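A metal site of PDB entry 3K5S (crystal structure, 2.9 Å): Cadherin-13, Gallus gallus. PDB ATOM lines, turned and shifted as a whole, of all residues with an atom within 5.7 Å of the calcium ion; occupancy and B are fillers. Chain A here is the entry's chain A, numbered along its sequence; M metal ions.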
ATOM      1  N   ASN A 101      13.966 -14.718 -14.365  1.00  0.00           N
ATOM      2  CA  ASN A 101      13.787 -16.169 -14.275  1.00  0.00           C
ATOM      3  C   ASN A 101      13.127 -16.791 -15.521  1.00  0.00           C
ATOM      4  O   ASN A 101      11.929 -17.027 -15.544  1.00  0.00           O
ATOM      5  CB  ASN A 101      12.981 -16.515 -13.018  1.00  0.00           C
ATOM      6  CG  ASN A 101      13.108 -17.979 -12.631  1.00  0.00           C
ATOM      7  OD1 ASN A 101      14.183 -18.566 -12.760  1.00  0.00           O
ATOM      8  ND2 ASN A 101      12.014 -18.576 -12.159  1.00  0.00           N
ATOM      9  N   ASP A 102      13.913 -17.064 -16.549  1.00  0.00           N
ATOM     10  CA  ASP A 102      13.350 -17.538 -17.800  1.00  0.00           C
ATOM     11  C   ASP A 102      13.923 -18.849 -18.274  1.00  0.00           C
ATOM     12  O   ASP A 102      13.755 -19.225 -19.432  1.00  0.00           O
ATOM     13  CB  ASP A 102      13.437 -16.470 -18.910  1.00  0.00           C
ATOM     14  CG  ASP A 102      14.864 -16.026 -19.199  1.00  0.00           C
ATOM     15  OD1 ASP A 102      15.809 -16.798 -18.941  1.00  0.00           O
ATOM     16  OD2 ASP A 102      15.020 -14.901 -19.704  1.00  0.00           O
ATOM     17  N   ASN A 103      14.593 -19.547 -17.388  1.00  0.00           N
ATOM     18  CA  ASN A 103      15.049 -20.878 -17.724  1.00  0.00           C
ATOM     19  C   ASN A 103      14.534 -21.870 -16.700  1.00  0.00           C
ATOM     20  O   ASN A 103      14.661 -21.645 -15.514  1.00  0.00           O
ATOM     21  CB  ASN A 103      16.568 -20.939 -17.809  1.00  0.00           C
ATOM     22  CG  ASN A 103      17.091 -20.444 -19.134  1.00  0.00           C
ATOM     23  OD1 ASN A 103      16.964 -21.127 -20.153  1.00  0.00           O
ATOM     24  ND2 ASN A 103      17.698 -19.267 -19.130  1.00  0.00           N
ATOM     25  N   ARG A 104      13.943 -22.954 -17.153  1.00  0.00           N
ATOM     26  CA  ARG A 104      13.362 -23.898 -16.203  1.00  0.00           C
ATOM     27  C   ARG A 104      14.428 -24.911 -15.777  1.00  0.00           C
ATOM     28  O   ARG A 104      15.229 -25.347 -16.595  1.00  0.00           O
ATOM     29  CB  ARG A 104      12.136 -24.566 -16.843  1.00  0.00           C
ATOM     30  CG  ARG A 104      11.770 -25.912 -16.261  1.00  0.00           C
ATOM     31  CD  ARG A 104      10.997 -26.749 -17.273  1.00  0.00           C
ATOM     32  NE  ARG A 104      10.138 -25.901 -18.099  1.00  0.00           N
ATOM     33  CZ  ARG A 104       8.946 -25.458 -17.717  1.00  0.00           C
ATOM     34  NH1 ARG A 104       8.470 -25.767 -16.510  1.00  0.00           N
ATOM     35  NH2 ARG A 104       8.223 -24.685 -18.537  1.00  0.00           N
ATOM     36  N   PRO A 105      14.459 -25.266 -14.476  1.00  0.00           N
ATOM     37  CA  PRO A 105      15.380 -26.313 -13.984  1.00  0.00           C
ATOM     38  C   PRO A 105      15.227 -27.617 -14.769  1.00  0.00           C
ATOM     39  O   PRO A 105      14.093 -28.048 -15.023  1.00  0.00           O
ATOM     40  CB  PRO A 105      14.904 -26.529 -12.536  1.00  0.00           C
ATOM     41  CG  PRO A 105      14.191 -25.309 -12.144  1.00  0.00           C
ATOM     42  CD  PRO A 105      13.600 -24.733 -13.407  1.00  0.00           C
ATOM     43  N   ASP A 133      20.322 -25.409 -13.992  1.00  0.00           N
ATOM     44  CA  ASP A 133      19.433 -24.282 -14.280  1.00  0.00           C
ATOM     45  C   ASP A 133      20.183 -23.155 -14.979  1.00  0.00           C
ATOM     46  O   ASP A 133      21.106 -22.578 -14.423  1.00  0.00           O
ATOM     47  CB  ASP A 133      18.824 -23.756 -12.978  1.00  0.00           C
ATOM     48  CG  ASP A 133      17.667 -22.826 -13.226  1.00  0.00           C
ATOM     49  OD1 ASP A 133      17.840 -21.822 -13.945  1.00  0.00           O
ATOM     50  OD2 ASP A 133      16.565 -23.105 -12.690  1.00  0.00           O
ATOM     51  N   ALA A 134      19.763 -22.832 -16.201  1.00  0.00           N
ATOM     52  CA  ALA A 134      20.500 -21.879 -17.018  1.00  0.00           C
ATOM     53  C   ALA A 134      20.620 -20.467 -16.432  1.00  0.00           C
ATOM     54  O   ALA A 134      21.422 -19.656 -16.905  1.00  0.00           O
ATOM     55  CB  ALA A 134      19.934 -21.817 -18.428  1.00  0.00           C
ATOM     56  N   ASP A 135      19.835 -20.170 -15.405  1.00  0.00           N
ATOM     57  CA  ASP A 135      19.789 -18.816 -14.842  1.00  0.00           C
ATOM     58  C   ASP A 135      20.938 -18.501 -13.867  1.00  0.00           C
ATOM     59  O   ASP A 135      21.914 -19.244 -13.799  1.00  0.00           O
ATOM     60  CB  ASP A 135      18.413 -18.522 -14.254  1.00  0.00           C
ATOM     61  CG  ASP A 135      17.330 -18.459 -15.329  1.00  0.00           C
ATOM     62  OD1 ASP A 135      17.657 -18.630 -16.518  1.00  0.00           O
ATOM     63  OD2 ASP A 135      16.150 -18.244 -15.000  1.00  0.00           O
ATOM     64  N   ASN A 141      16.736 -17.178  -9.197  1.00  0.00           N
ATOM     65  CA  ASN A 141      16.218 -17.692 -10.442  1.00  0.00           C
ATOM     66  C   ASN A 141      16.767 -19.089 -10.695  1.00  0.00           C
ATOM     67  O   ASN A 141      16.066 -19.953 -11.175  1.00  0.00           O
ATOM     68  CB  ASN A 141      16.445 -16.699 -11.562  1.00  0.00           C
ATOM     69  CG  ASN A 141      15.824 -15.341 -11.269  1.00  0.00           C
ATOM     70  OD1 ASN A 141      15.073 -15.191 -10.308  1.00  0.00           O
ATOM     71  ND2 ASN A 141      16.130 -14.362 -12.095  1.00  0.00           N
ATOM     72  N   ALA A 142      18.033 -19.303 -10.351  1.00  0.00           N
ATOM     73  CA  ALA A 142      18.510 -20.634 -10.016  1.00  0.00           C
ATOM     74  C   ALA A 142      18.505 -20.608  -8.494  1.00  0.00           C
ATOM     75  O   ALA A 142      17.966 -19.682  -7.926  1.00  0.00           O
ATOM     76  CB  ALA A 142      19.892 -20.874 -10.558  1.00  0.00           C
ATOM     77  N   LEU A 144      17.924 -24.059  -6.430  1.00  0.00           N
ATOM     78  CA  LEU A 144      16.919 -25.084  -6.543  1.00  0.00           C
ATOM     79  C   LEU A 144      16.658 -25.781  -5.199  1.00  0.00           C
ATOM     80  O   LEU A 144      17.543 -25.873  -4.338  1.00  0.00           O
ATOM     81  CB  LEU A 144      17.348 -26.086  -7.615  1.00  0.00           C
ATOM     82  CG  LEU A 144      18.047 -25.490  -8.853  1.00  0.00           C
ATOM     83  CD1 LEU A 144      18.210 -26.543  -9.942  1.00  0.00           C
ATOM     84  CD2 LEU A 144      17.348 -24.257  -9.425  1.00  0.00           C
ATOM     85  N   ASP A 197      12.623 -23.900  -8.601  1.00  0.00           N
ATOM     86  CA  ASP A 197      13.299 -22.600  -8.564  1.00  0.00           C
ATOM     87  C   ASP A 197      12.987 -21.785  -7.315  1.00  0.00           C
ATOM     88  O   ASP A 197      12.183 -22.192  -6.474  1.00  0.00           O
ATOM     89  CB  ASP A 197      12.807 -21.754  -9.727  1.00  0.00           C
ATOM     90  CG  ASP A 197      13.746 -21.741 -10.858  1.00  0.00           C
ATOM     91  OD1 ASP A 197      14.845 -22.314 -10.700  1.00  0.00           O
ATOM     92  OD2 ASP A 197      13.385 -21.151 -11.886  1.00  0.00           O
ATOM     93  N   LEU A 205       9.651 -22.546 -10.897  1.00  0.00           N
ATOM     94  CA  LEU A 205       9.473 -23.349 -12.098  1.00  0.00           C
ATOM     95  C   LEU A 205      10.065 -24.713 -11.783  1.00  0.00           C
ATOM     96  O   LEU A 205      10.918 -24.818 -10.902  1.00  0.00           O
ATOM     97  CB  LEU A 205      10.197 -22.713 -13.288  1.00  0.00           C
ATOM     98  CG  LEU A 205       9.631 -21.407 -13.859  1.00  0.00           C
ATOM     99  CD1 LEU A 205      10.729 -20.624 -14.558  1.00  0.00           C
ATOM    100  CD2 LEU A 205       8.438 -21.668 -14.788  1.00  0.00           C
HETATM  101 CA    CA M   1      15.408 -20.775 -13.407  1.00  0.00          CA
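N of Asn 103 is in hydrogen-bond range of OD2 of Asp 135 (3.1 Å).
The side-chain amide nitrogen (ND2) of Asn 103 sits close to the side-chain carboxylate (OD1) of Asp 102, at 3.1 Å.
N of Asp 197 is in hydrogen-bond range of O of Leu 205.
The side-chain carboxylate (OD2) of Asp 135 lies close to the side-chain amide oxygen (OD1) of Asn 101 (3.0 Å).
The backbone NH (N) of Asp 135 sits close to the side-chain carboxylate (OD1) of Asp 133, at 3.0 Å.
The nearest printed residue that does not touch the calcium ion is Ala 142 (4.3 Å).
The backbone carbonyl oxygen (O) of Asn 103 is bound to the calcium ion, at 2.4 Å.
O of Asn 141 is bound to the calcium ion (2.5 Å).
OD2 of Asp 197 is bound to the calcium ion (2.6 Å).
OD1 of Asn 101 binds the calcium ion (2.6 Å).
OD2 of Asp 133 binds the calcium ion.
The calcium ion is bound by the side-chain carboxylate (OD1) of Asp 133 (2.7 Å).
Slightly farther from the calcium ion lies the side-chain carboxylate (OD2) of Asp 135 (3.1 Å).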
